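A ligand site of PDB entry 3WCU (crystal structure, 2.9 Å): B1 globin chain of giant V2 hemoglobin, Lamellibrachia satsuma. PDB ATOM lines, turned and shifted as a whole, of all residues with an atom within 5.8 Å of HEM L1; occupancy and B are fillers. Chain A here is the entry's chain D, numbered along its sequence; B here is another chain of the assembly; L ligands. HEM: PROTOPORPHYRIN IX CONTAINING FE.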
ATOM      1  N   LEU A  40      -4.533  39.712   1.603  1.00  0.00           N
ATOM      2  CA  LEU A  40      -5.057  38.806   0.591  1.00  0.00           C
ATOM      3  C   LEU A  40      -6.517  38.541   0.927  1.00  0.00           C
ATOM      4  O   LEU A  40      -7.398  38.571   0.064  1.00  0.00           O
ATOM      5  CB  LEU A  40      -4.286  37.493   0.618  1.00  0.00           C
ATOM      6  CG  LEU A  40      -4.877  36.243  -0.021  1.00  0.00           C
ATOM      7  CD1 LEU A  40      -5.211  36.483  -1.480  1.00  0.00           C
ATOM      8  CD2 LEU A  40      -3.879  35.124   0.120  1.00  0.00           C
ATOM      9  N   SER A  47     -11.266  33.058   0.214  1.00  0.00           N
ATOM     10  CA  SER A  47     -10.093  32.199   0.118  1.00  0.00           C
ATOM     11  C   SER A  47      -9.538  31.818   1.482  1.00  0.00           C
ATOM     12  O   SER A  47      -8.779  30.848   1.592  1.00  0.00           O
ATOM     13  CB  SER A  47      -9.000  32.919  -0.673  1.00  0.00           C
ATOM     14  OG  SER A  47      -8.546  34.072   0.015  1.00  0.00           O
ATOM     15  N   LEU A  50      -9.407  28.133   2.686  1.00  0.00           N
ATOM     16  CA  LEU A  50      -8.476  27.177   2.113  1.00  0.00           C
ATOM     17  C   LEU A  50      -7.341  26.791   3.038  1.00  0.00           C
ATOM     18  O   LEU A  50      -6.721  25.736   2.884  1.00  0.00           O
ATOM     19  CB  LEU A  50      -7.896  27.724   0.814  1.00  0.00           C
ATOM     20  CG  LEU A  50      -8.826  27.621  -0.390  1.00  0.00           C
ATOM     21  CD1 LEU A  50      -8.278  28.449  -1.542  1.00  0.00           C
ATOM     22  CD2 LEU A  50      -8.985  26.157  -0.775  1.00  0.00           C
ATOM     23  N   PHE A  51      -7.091  27.642   4.028  1.00  0.00           N
ATOM     24  CA  PHE A  51      -5.993  27.412   4.965  1.00  0.00           C
ATOM     25  C   PHE A  51      -6.413  26.816   6.307  1.00  0.00           C
ATOM     26  O   PHE A  51      -6.059  27.327   7.358  1.00  0.00           O
ATOM     27  CB  PHE A  51      -5.228  28.734   5.173  1.00  0.00           C
ATOM     28  CG  PHE A  51      -4.958  29.486   3.891  1.00  0.00           C
ATOM     29  CD1 PHE A  51      -5.570  30.718   3.637  1.00  0.00           C
ATOM     30  CD2 PHE A  51      -4.138  28.934   2.904  1.00  0.00           C
ATOM     31  CE1 PHE A  51      -5.386  31.375   2.422  1.00  0.00           C
ATOM     32  CE2 PHE A  51      -3.948  29.584   1.685  1.00  0.00           C
ATOM     33  CZ  PHE A  51      -4.571  30.809   1.449  1.00  0.00           C
ATOM     34  N   ASN A  52      -7.148  25.709   6.271  1.00  0.00           N
ATOM     35  CA  ASN A  52      -7.580  25.057   7.500  1.00  0.00           C
ATOM     36  C   ASN A  52      -6.435  24.324   8.167  1.00  0.00           C
ATOM     37  O   ASN A  52      -6.073  24.621   9.299  1.00  0.00           O
ATOM     38  CB  ASN A  52      -8.730  24.093   7.247  1.00  0.00           C
ATOM     39  CG  ASN A  52     -10.057  24.801   7.067  1.00  0.00           C
ATOM     40  OD1 ASN A  52     -10.428  25.644   7.873  1.00  0.00           O
ATOM     41  ND2 ASN A  52     -10.770  24.458   5.997  1.00  0.00           N
ATOM     42  N   ASN A  53      -5.858  23.364   7.453  1.00  0.00           N
ATOM     43  CA  ASN A  53      -4.733  22.598   7.985  1.00  0.00           C
ATOM     44  C   ASN A  53      -3.708  23.484   8.677  1.00  0.00           C
ATOM     45  O   ASN A  53      -3.221  23.156   9.758  1.00  0.00           O
ATOM     46  CB  ASN A  53      -4.038  21.820   6.871  1.00  0.00           C
ATOM     47  CG  ASN A  53      -4.792  20.580   6.489  1.00  0.00           C
ATOM     48  OD1 ASN A  53      -6.015  20.607   6.356  1.00  0.00           O
ATOM     49  ND2 ASN A  53      -4.062  19.482   6.299  1.00  0.00           N
ATOM     50  N   VAL A  54      -3.372  24.599   8.046  1.00  0.00           N
ATOM     51  CA  VAL A  54      -2.386  25.492   8.606  1.00  0.00           C
ATOM     52  C   VAL A  54      -2.933  26.374   9.723  1.00  0.00           C
ATOM     53  O   VAL A  54      -2.319  27.381  10.079  1.00  0.00           O
ATOM     54  CB  VAL A  54      -1.777  26.377   7.498  1.00  0.00           C
ATOM     55  CG1 VAL A  54      -1.292  25.501   6.355  1.00  0.00           C
ATOM     56  CG2 VAL A  54      -2.807  27.376   7.021  1.00  0.00           C
ATOM     57  N   HIS A  67       3.455  28.094   7.433  1.00  0.00           N
ATOM     58  CA  HIS A  67       2.842  28.061   6.109  1.00  0.00           C
ATOM     59  C   HIS A  67       3.136  29.307   5.294  1.00  0.00           C
ATOM     60  O   HIS A  67       3.410  29.214   4.098  1.00  0.00           O
ATOM     61  CB  HIS A  67       1.340  27.881   6.217  1.00  0.00           C
ATOM     62  CG  HIS A  67       0.628  28.180   4.939  1.00  0.00           C
ATOM     63  ND1 HIS A  67       0.582  27.280   3.895  1.00  0.00           N
ATOM     64  CD2 HIS A  67      -0.024  29.287   4.525  1.00  0.00           C
ATOM     65  CE1 HIS A  67      -0.078  27.827   2.884  1.00  0.00           C
ATOM     66  NE2 HIS A  67      -0.457  29.044   3.239  1.00  0.00           N
ATOM     67  N   ARG A  70       6.699  29.002   4.175  1.00  0.00           N
ATOM     68  CA  ARG A  70       6.999  28.149   3.039  1.00  0.00           C
ATOM     69  C   ARG A  70       6.359  28.652   1.738  1.00  0.00           C
ATOM     70  O   ARG A  70       6.720  28.221   0.643  1.00  0.00           O
ATOM     71  CB  ARG A  70       6.662  26.674   3.325  1.00  0.00           C
ATOM     72  CG  ARG A  70       5.359  26.379   4.007  1.00  0.00           C
ATOM     73  CD  ARG A  70       5.277  24.886   4.240  1.00  0.00           C
ATOM     74  NE  ARG A  70       5.032  24.554   5.633  1.00  0.00           N
ATOM     75  CZ  ARG A  70       3.836  24.588   6.222  1.00  0.00           C
ATOM     76  NH1 ARG A  70       2.753  24.932   5.541  1.00  0.00           N
ATOM     77  NH2 ARG A  70       3.732  24.261   7.507  1.00  0.00           N
ATOM     78  N   VAL A  71       5.412  29.582   1.858  1.00  0.00           N
ATOM     79  CA  VAL A  71       4.803  30.160   0.667  1.00  0.00           C
ATOM     80  C   VAL A  71       5.837  31.198   0.203  1.00  0.00           C
ATOM     81  O   VAL A  71       6.287  31.189  -0.944  1.00  0.00           O
ATOM     82  CB  VAL A  71       3.502  30.920   0.983  1.00  0.00           C
ATOM     83  CG1 VAL A  71       3.029  31.656  -0.256  1.00  0.00           C
ATOM     84  CG2 VAL A  71       2.442  29.962   1.472  1.00  0.00           C
ATOM     85  N   LEU A  72       6.185  32.100   1.116  1.00  0.00           N
ATOM     86  CA  LEU A  72       7.164  33.119   0.830  1.00  0.00           C
ATOM     87  C   LEU A  72       8.520  32.496   0.520  1.00  0.00           C
ATOM     88  O   LEU A  72       9.322  33.095  -0.194  1.00  0.00           O
ATOM     89  CB  LEU A  72       7.279  34.101   2.003  1.00  0.00           C
ATOM     90  CG  LEU A  72       6.108  35.063   2.197  1.00  0.00           C
ATOM     91  CD1 LEU A  72       6.515  36.135   3.163  1.00  0.00           C
ATOM     92  CD2 LEU A  72       5.708  35.717   0.888  1.00  0.00           C
ATOM     93  N   GLY A  74       8.899  29.769  -1.194  1.00  0.00           N
ATOM     94  CA  GLY A  74       8.760  29.296  -2.568  1.00  0.00           C
ATOM     95  C   GLY A  74       8.858  30.476  -3.506  1.00  0.00           C
ATOM     96  O   GLY A  74       9.383  30.360  -4.619  1.00  0.00           O
ATOM     97  N   LEU A  75       8.348  31.625  -3.072  1.00  0.00           N
ATOM     98  CA  LEU A  75       8.427  32.837  -3.859  1.00  0.00           C
ATOM     99  C   LEU A  75       9.851  33.407  -3.730  1.00  0.00           C
ATOM    100  O   LEU A  75      10.215  34.343  -4.438  1.00  0.00           O
ATOM    101  CB  LEU A  75       7.423  33.863  -3.353  1.00  0.00           C
ATOM    102  CG  LEU A  75       7.632  35.260  -3.923  1.00  0.00           C
ATOM    103  CD1 LEU A  75       7.250  35.296  -5.393  1.00  0.00           C
ATOM    104  CD2 LEU A  75       6.816  36.254  -3.135  1.00  0.00           C
ATOM    105  N   LEU A  95       5.040  23.682  -8.916  1.00  0.00           N
ATOM    106  CA  LEU A  95       4.162  24.445  -8.029  1.00  0.00           C
ATOM    107  C   LEU A  95       2.710  24.522  -8.525  1.00  0.00           C
ATOM    108  O   LEU A  95       1.785  24.748  -7.740  1.00  0.00           O
ATOM    109  CB  LEU A  95       4.695  25.866  -7.811  1.00  0.00           C
ATOM    110  CG  LEU A  95       5.816  26.005  -6.784  1.00  0.00           C
ATOM    111  CD1 LEU A  95       6.511  27.334  -6.972  1.00  0.00           C
ATOM    112  CD2 LEU A  95       5.267  25.871  -5.378  1.00  0.00           C
ATOM    113  N   GLN A  98       0.726  21.263  -7.798  1.00  0.00           N
ATOM    114  CA  GLN A  98       0.243  21.239  -6.423  1.00  0.00           C
ATOM    115  C   GLN A  98      -0.949  22.160  -6.175  1.00  0.00           C
ATOM    116  O   GLN A  98      -1.968  21.722  -5.657  1.00  0.00           O
ATOM    117  CB  GLN A  98       1.364  21.606  -5.461  1.00  0.00           C
ATOM    118  CG  GLN A  98       2.635  20.826  -5.721  1.00  0.00           C
ATOM    119  CD  GLN A  98       3.699  21.098  -4.697  1.00  0.00           C
ATOM    120  OE1 GLN A  98       3.847  22.237  -4.228  1.00  0.00           O
ATOM    121  NE2 GLN A  98       4.469  20.065  -4.345  1.00  0.00           N
ATOM    122  N   HIS A  99      -0.829  23.438  -6.531  1.00  0.00           N
ATOM    123  CA  HIS A  99      -1.930  24.369  -6.287  1.00  0.00           C
ATOM    124  C   HIS A  99      -3.199  23.997  -7.059  1.00  0.00           C
ATOM    125  O   HIS A  99      -4.295  24.457  -6.740  1.00  0.00           O
ATOM    126  CB  HIS A  99      -1.485  25.805  -6.592  1.00  0.00           C
ATOM    127  CG  HIS A  99      -0.569  26.373  -5.557  1.00  0.00           C
ATOM    128  ND1 HIS A  99       0.653  25.814  -5.266  1.00  0.00           N
ATOM    129  CD2 HIS A  99      -0.748  27.380  -4.663  1.00  0.00           C
ATOM    130  CE1 HIS A  99       1.192  26.450  -4.239  1.00  0.00           C
ATOM    131  NE2 HIS A  99       0.360  27.398  -3.854  1.00  0.00           N
ATOM    132  N   ARG A 102      -5.102  20.766  -5.770  1.00  0.00           N
ATOM    133  CA  ARG A 102      -5.719  21.210  -4.527  1.00  0.00           C
ATOM    134  C   ARG A 102      -7.058  21.826  -4.926  1.00  0.00           C
ATOM    135  O   ARG A 102      -7.142  22.559  -5.923  1.00  0.00           O
ATOM    136  CB  ARG A 102      -4.836  22.234  -3.831  1.00  0.00           C
ATOM    137  CG  ARG A 102      -5.174  22.391  -2.367  1.00  0.00           C
ATOM    138  CD  ARG A 102      -3.921  22.673  -1.573  1.00  0.00           C
ATOM    139  NE  ARG A 102      -3.915  21.947  -0.310  1.00  0.00           N
ATOM    140  CZ  ARG A 102      -4.848  22.069   0.641  1.00  0.00           C
ATOM    141  NH1 ARG A 102      -4.740  21.351   1.759  1.00  0.00           N
ATOM    142  NH2 ARG A 102      -5.878  22.898   0.483  1.00  0.00           N
ATOM    143  N   LEU A 105      -9.007  26.303  -5.333  1.00  0.00           N
ATOM    144  CA  LEU A 105      -8.090  27.382  -5.679  1.00  0.00           C
ATOM    145  C   LEU A 105      -8.390  28.014  -7.023  1.00  0.00           C
ATOM    146  O   LEU A 105      -8.167  27.389  -8.063  1.00  0.00           O
ATOM    147  CB  LEU A 105      -6.641  26.886  -5.669  1.00  0.00           C
ATOM    148  CG  LEU A 105      -5.872  27.141  -4.369  1.00  0.00           C
ATOM    149  CD1 LEU A 105      -6.127  26.023  -3.377  1.00  0.00           C
ATOM    150  CD2 LEU A 105      -4.399  27.229  -4.672  1.00  0.00           C
ATOM    151  N   TYR A 109      -7.522  34.173  -7.385  1.00  0.00           N
ATOM    152  CA  TYR A 109      -6.957  34.286  -6.042  1.00  0.00           C
ATOM    153  C   TYR A 109      -5.502  34.728  -6.152  1.00  0.00           C
ATOM    154  O   TYR A 109      -5.055  35.617  -5.421  1.00  0.00           O
ATOM    155  CB  TYR A 109      -7.042  32.944  -5.296  1.00  0.00           C
ATOM    156  CG  TYR A 109      -8.431  32.561  -4.824  1.00  0.00           C
ATOM    157  CD1 TYR A 109      -9.295  33.515  -4.289  1.00  0.00           C
ATOM    158  CD2 TYR A 109      -8.865  31.236  -4.892  1.00  0.00           C
ATOM    159  CE1 TYR A 109     -10.567  33.156  -3.830  1.00  0.00           C
ATOM    160  CE2 TYR A 109     -10.125  30.865  -4.442  1.00  0.00           C
ATOM    161  CZ  TYR A 109     -10.971  31.828  -3.919  1.00  0.00           C
ATOM    162  OH  TYR A 109     -12.221  31.463  -3.487  1.00  0.00           O
ATOM    163  N   PHE A 110      -4.764  34.108  -7.059  1.00  0.00           N
ATOM    164  CA  PHE A 110      -3.372  34.472  -7.251  1.00  0.00           C
ATOM    165  C   PHE A 110      -3.286  35.920  -7.681  1.00  0.00           C
ATOM    166  O   PHE A 110      -2.460  36.673  -7.177  1.00  0.00           O
ATOM    167  CB  PHE A 110      -2.715  33.566  -8.272  1.00  0.00           C
ATOM    168  CG  PHE A 110      -2.123  32.329  -7.659  1.00  0.00           C
ATOM    169  CD1 PHE A 110      -2.953  31.342  -7.127  1.00  0.00           C
ATOM    170  CD2 PHE A 110      -0.749  32.153  -7.593  1.00  0.00           C
ATOM    171  CE1 PHE A 110      -2.411  30.199  -6.539  1.00  0.00           C
ATOM    172  CE2 PHE A 110      -0.198  31.010  -7.016  1.00  0.00           C
ATOM    173  CZ  PHE A 110      -1.032  30.037  -6.487  1.00  0.00           C
ATOM    174  N   MET A 113      -3.237  37.781  -4.823  1.00  0.00           N
ATOM    175  CA  MET A 113      -1.925  37.715  -4.175  1.00  0.00           C
ATOM    176  C   MET A 113      -0.929  38.645  -4.867  1.00  0.00           C
ATOM    177  O   MET A 113      -0.058  39.236  -4.219  1.00  0.00           O
ATOM    178  CB  MET A 113      -1.383  36.279  -4.208  1.00  0.00           C
ATOM    179  CG  MET A 113       0.023  36.114  -3.667  1.00  0.00           C
ATOM    180  SD  MET A 113       0.146  36.347  -1.891  1.00  0.00           S
ATOM    181  CE  MET A 113      -0.219  34.699  -1.297  1.00  0.00           C
ATOM    182  N   LEU A 117       1.070  41.744  -2.979  1.00  0.00           N
ATOM    183  CA  LEU A 117       2.514  41.895  -2.989  1.00  0.00           C
ATOM    184  C   LEU A 117       2.895  43.240  -3.585  1.00  0.00           C
ATOM    185  O   LEU A 117       3.662  43.995  -2.983  1.00  0.00           O
ATOM    186  CB  LEU A 117       3.156  40.777  -3.807  1.00  0.00           C
ATOM    187  CG  LEU A 117       3.206  39.388  -3.165  1.00  0.00           C
ATOM    188  CD1 LEU A 117       3.681  38.361  -4.187  1.00  0.00           C
ATOM    189  CD2 LEU A 117       4.130  39.424  -1.984  1.00  0.00           C
ATOM    190  N   LYS A 141       3.502  34.373 -11.443  1.00  0.00           N
ATOM    191  CA  LYS A 141       2.108  34.118 -11.077  1.00  0.00           C
ATOM    192  C   LYS A 141       1.482  33.151 -12.094  1.00  0.00           C
ATOM    193  O   LYS A 141       1.237  31.980 -11.773  1.00  0.00           O
ATOM    194  CB  LYS A 141       1.306  35.410 -11.050  1.00  0.00           C
ATOM    195  CG  LYS A 141      -0.174  35.229 -10.753  1.00  0.00           C
ATOM    196  CD  LYS A 141      -1.056  36.109 -11.639  1.00  0.00           C
ATOM    197  CE  LYS A 141      -0.856  37.614 -11.371  1.00  0.00           C
ATOM    198  NZ  LYS A 141      -1.741  38.495 -12.215  1.00  0.00           N
ATOM    199  N   ILE A 144       2.817  29.682 -12.129  1.00  0.00           N
ATOM    200  CA  ILE A 144       2.459  28.902 -10.944  1.00  0.00           C
ATOM    201  C   ILE A 144       0.991  28.507 -10.990  1.00  0.00           C
ATOM    202  O   ILE A 144       0.634  27.346 -10.792  1.00  0.00           O
ATOM    203  CB  ILE A 144       2.665  29.696  -9.640  1.00  0.00           C
ATOM    204  CG1 ILE A 144       4.138  29.912  -9.367  1.00  0.00           C
ATOM    205  CG2 ILE A 144       2.029  28.964  -8.479  1.00  0.00           C
ATOM    206  CD1 ILE A 144       4.409  30.741  -8.137  1.00  0.00           C
ATOM    207  N   HIS B  89       5.840  19.357   9.367  1.00  0.00           N
ATOM    208  CA  HIS B  89       5.275  19.304   8.025  1.00  0.00           C
ATOM    209  C   HIS B  89       6.202  18.569   7.052  1.00  0.00           C
ATOM    210  O   HIS B  89       5.745  17.936   6.109  1.00  0.00           O
ATOM    211  CB  HIS B  89       5.006  20.741   7.532  1.00  0.00           C
ATOM    212  CG  HIS B  89       4.507  20.823   6.126  1.00  0.00           C
ATOM    213  ND1 HIS B  89       3.600  19.936   5.597  1.00  0.00           N
ATOM    214  CD2 HIS B  89       4.775  21.721   5.140  1.00  0.00           C
ATOM    215  CE1 HIS B  89       3.318  20.277   4.349  1.00  0.00           C
ATOM    216  NE2 HIS B  89       4.021  21.354   4.049  1.00  0.00           N
ATOM    217  N   GLN B  93       6.133  14.667   4.871  1.00  0.00           N
ATOM    218  CA  GLN B  93       6.442  14.617   3.457  1.00  0.00           C
ATOM    219  C   GLN B  93       7.577  13.616   3.228  1.00  0.00           C
ATOM    220  O   GLN B  93       7.642  12.946   2.197  1.00  0.00           O
ATOM    221  CB  GLN B  93       6.835  16.011   2.941  1.00  0.00           C
ATOM    222  CG  GLN B  93       5.786  17.100   3.181  1.00  0.00           C
ATOM    223  CD  GLN B  93       6.101  18.415   2.495  1.00  0.00           C
ATOM    224  OE1 GLN B  93       7.179  18.989   2.664  1.00  0.00           O
ATOM    225  NE2 GLN B  93       5.163  18.911   1.720  1.00  0.00           N
HETATM  226  CHA HEM L   1       0.631  25.597  -0.351  1.00  0.00           C
HETATM  227  CHB HEM L   1       3.559  28.600  -2.580  1.00  0.00           C
HETATM  228  CHC HEM L   1      -0.136  31.520  -3.689  1.00  0.00           C
HETATM  229  CHD HEM L   1      -3.106  28.411  -1.518  1.00  0.00           C
HETATM  230  C1A HEM L   1       1.783  26.165  -0.859  1.00  0.00           C
HETATM  231  C2A HEM L   1       3.057  25.607  -0.678  1.00  0.00           C
HETATM  232  C3A HEM L   1       3.887  26.438  -1.317  1.00  0.00           C
HETATM  233  C4A HEM L   1       3.117  27.547  -1.894  1.00  0.00           C
HETATM  234  CMA HEM L   1       5.416  26.305  -1.418  1.00  0.00           C
HETATM  235  CAA HEM L   1       3.448  24.372   0.087  1.00  0.00           C
HETATM  236  CBA HEM L   1       3.322  23.054  -0.560  1.00  0.00           C
HETATM  237  CGA HEM L   1       3.756  21.950   0.428  1.00  0.00           C
HETATM  238  O1A HEM L   1       3.060  21.755   1.476  1.00  0.00           O
HETATM  239  O2A HEM L   1       4.769  21.324   0.196  1.00  0.00           O
HETATM  240  C1B HEM L   1       2.822  29.714  -3.099  1.00  0.00           C
HETATM  241  C2B HEM L   1       3.419  30.831  -3.804  1.00  0.00           C
HETATM  242  C3B HEM L   1       2.300  31.695  -4.112  1.00  0.00           C
HETATM  243  C4B HEM L   1       1.161  31.026  -3.596  1.00  0.00           C
HETATM  244  CMB HEM L   1       4.868  31.033  -4.105  1.00  0.00           C
HETATM  245  CAB HEM L   1       2.421  32.959  -4.807  1.00  0.00           C
HETATM  246  CBB HEM L   1       2.718  33.091  -6.079  1.00  0.00           C
HETATM  247  C1C HEM L   1      -1.269  30.902  -3.195  1.00  0.00           C
HETATM  248  C2C HEM L   1      -2.605  31.486  -3.341  1.00  0.00           C
HETATM  249  C3C HEM L   1      -3.505  30.601  -2.719  1.00  0.00           C
HETATM  250  C4C HEM L   1      -2.617  29.478  -2.205  1.00  0.00           C
HETATM  251  CMC HEM L   1      -2.920  32.818  -4.033  1.00  0.00           C
HETATM  252  CAC HEM L   1      -4.854  30.729  -2.610  1.00  0.00           C
HETATM  253  CBC HEM L   1      -5.722  31.468  -2.012  1.00  0.00           C
HETATM  254  C1D HEM L   1      -2.344  27.370  -1.006  1.00  0.00           C
HETATM  255  C2D HEM L   1      -2.936  26.212  -0.211  1.00  0.00           C
HETATM  256  C3D HEM L   1      -1.847  25.411   0.120  1.00  0.00           C
HETATM  257  C4D HEM L   1      -0.653  26.074  -0.469  1.00  0.00           C
HETATM  258  CMD HEM L   1      -4.413  26.050   0.105  1.00  0.00           C
HETATM  259  CAD HEM L   1      -1.848  24.106   0.926  1.00  0.00           C
HETATM  260  CBD HEM L   1      -1.728  24.359   2.422  1.00  0.00           C
HETATM  261  CGD HEM L   1      -1.700  23.133   3.285  1.00  0.00           C
HETATM  262  O1D HEM L   1      -0.867  22.204   3.032  1.00  0.00           O
HETATM  263  O2D HEM L   1      -2.474  23.042   4.252  1.00  0.00           O
HETATM  264  NA  HEM L   1       1.798  27.366  -1.604  1.00  0.00           N
HETATM  265  NB  HEM L   1       1.498  29.802  -2.965  1.00  0.00           N
HETATM  266  NC  HEM L   1      -1.325  29.691  -2.514  1.00  0.00           N
HETATM  267  ND  HEM L   1      -1.007  27.252  -1.123  1.00  0.00           N
HETATM  268 FE   HEM L   1       0.223  28.529  -2.077  1.00  0.00          FE
HETATM  269  CHA HEM L   2      11.865  16.044  -1.418  1.00  0.00           C
HETATM  270  CHB HEM L   2      13.425  19.184   1.764  1.00  0.00           C
HETATM  271  CHC HEM L   2      16.893  16.112   3.170  1.00  0.00           C
HETATM  272  CHD HEM L   2      15.228  12.952  -0.035  1.00  0.00           C
HETATM  273  C1A HEM L   2      11.979  17.187  -0.686  1.00  0.00           C
HETATM  274  C2A HEM L   2      11.167  18.305  -0.885  1.00  0.00           C
HETATM  275  C3A HEM L   2      11.590  19.214   0.029  1.00  0.00           C
HETATM  276  C4A HEM L   2      12.692  18.636   0.790  1.00  0.00           C
HETATM  277  CMA HEM L   2      11.071  20.632   0.278  1.00  0.00           C
HETATM  278  CAA HEM L   2      10.062  18.403  -1.950  1.00  0.00           C
HETATM  279  CBA HEM L   2       8.753  19.045  -1.607  1.00  0.00           C
HETATM  280  CGA HEM L   2       7.776  19.088  -2.798  1.00  0.00           C
HETATM  281  O1A HEM L   2       7.733  18.120  -3.625  1.00  0.00           O
HETATM  282  O2A HEM L   2       7.094  20.069  -2.932  1.00  0.00           O
HETATM  283  C1B HEM L   2      14.530  18.633   2.466  1.00  0.00           C
HETATM  284  C2B HEM L   2      15.275  19.337   3.494  1.00  0.00           C
HETATM  285  C3B HEM L   2      16.305  18.405   3.894  1.00  0.00           C
HETATM  286  C4B HEM L   2      16.107  17.255   3.102  1.00  0.00           C
HETATM  287  CMB HEM L   2      15.010  20.714   3.993  1.00  0.00           C
HETATM  288  CAB HEM L   2      17.302  18.691   4.896  1.00  0.00           C
HETATM  289  CBB HEM L   2      17.044  18.966   6.158  1.00  0.00           C
HETATM  290  C1C HEM L   2      16.724  14.966   2.390  1.00  0.00           C
HETATM  291  C2C HEM L   2      17.602  13.790   2.496  1.00  0.00           C
HETATM  292  C3C HEM L   2      17.134  12.843   1.575  1.00  0.00           C
HETATM  293  C4C HEM L   2      15.956  13.533   0.927  1.00  0.00           C
HETATM  294  CMC HEM L   2      18.792  13.640   3.438  1.00  0.00           C
HETATM  295  CAC HEM L   2      17.634  11.612   1.315  1.00  0.00           C
HETATM  296  CBC HEM L   2      18.451  11.021   0.517  1.00  0.00           C
HETATM  297  C1D HEM L   2      14.158  13.506  -0.696  1.00  0.00           C
HETATM  298  C2D HEM L   2      13.392  12.813  -1.791  1.00  0.00           C
HETATM  299  C3D HEM L   2      12.439  13.711  -2.171  1.00  0.00           C
HETATM  300  C4D HEM L   2      12.618  14.917  -1.331  1.00  0.00           C
HETATM  301  CMD HEM L   2      13.700  11.400  -2.312  1.00  0.00           C
HETATM  302  CAD HEM L   2      11.390  13.543  -3.261  1.00  0.00           C
HETATM  303  CBD HEM L   2      11.816  14.182  -4.546  1.00  0.00           C
HETATM  304  CGD HEM L   2      10.821  14.061  -5.632  1.00  0.00           C
HETATM  305  O1D HEM L   2      10.739  12.987  -6.287  1.00  0.00           O
HETATM  306  O2D HEM L   2      10.074  15.036  -5.890  1.00  0.00           O
HETATM  307  NA  HEM L   2      12.929  17.372   0.333  1.00  0.00           N
HETATM  308  NB  HEM L   2      15.002  17.411   2.220  1.00  0.00           N
HETATM  309  NC  HEM L   2      15.741  14.753   1.433  1.00  0.00           N
HETATM  310  ND  HEM L   2      13.652  14.741  -0.448  1.00  0.00           N
HETATM  311 FE   HEM L   2      14.319  16.047   0.906  1.00  0.00          FE
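Ser 47 touches HEM L1 (CB to CBC, 3.8 Å). Leu 50 touches HEM L1 (O to CMD, 3.6 Å). Phe 51 touches HEM L1 (CE2 to CHD, 3.5 Å). Asn 53 touches HEM L1. CG1 of Val 54 touches O2D of HEM L1 (3.4 Å). His 67 touches HEM L1. O of Arg 70 touches CMA of HEM L1 (3.1 Å). CG1 of Val 71 touches C1B of HEM L1, at 3.4 Å. Leu 75 touches HEM L1 (N to CMB, 3.7 Å). Leu 95 touches HEM L1. Gln 98 touches HEM L1. CD2 of Leu 105 touches CHD of HEM L1, at 3.6 Å. Tyr 109 touches HEM L1. Phe 110 touches HEM L1. Met 113 touches HEM L1. Ile 144 touches HEM L1 (CD1 to CBB, 3.6 Å). Hydrophobic or aromatic side chains that line HEM L1: Leu 50, Phe 51, Val 54, His 67, Val 71, Leu 75, Leu 95, His 99, Leu 105, Tyr 109, Phe 110, Met 113, Ile 144 and His 89 of chain B. 20 residues have an atom within 4 Å of HEM L1: Ser 47, Leu 50, Phe 51, Asn 53, Val 54, His 67, Arg 70, Val 71, Leu 75, Leu 95, Gln 98, His 99, Arg 102, Leu 105, Tyr 109, Phe 110, Met 113, Ile 144, His 89 of chain B and Gln 93 of chain B. The nearest printed residue that does not touch HEM L1 is Gly 74 (4.1 Å).
A ring nitrogen (ND1) of His 99 is in hydrogen-bond range of the backbone carbonyl oxygen of Leu 95, 2.9 Å away.
A ring nitrogen (NE2) of His 99 is bound to an iron atom (FE) of HEM L1 (2.1 Å). An oxygen (O1A) of HEM L1 lies within hydrogen-bond range of a ring nitrogen (NE2) of His 89 of chain B, 2.8 Å away. The side-chain amide nitrogen of Gln 93 of chain B is in hydrogen-bond range of an oxygen (O2A) of HEM L1 (2.9 Å). The guanidinium group of Arg 102 lies within salt-bridge range of an oxygen (O2D) of HEM L1, at 3.8 Å. NE2 of Gln 98 sits at hydrogen-bond distance from O2A of HEM L2 (3.0 Å).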
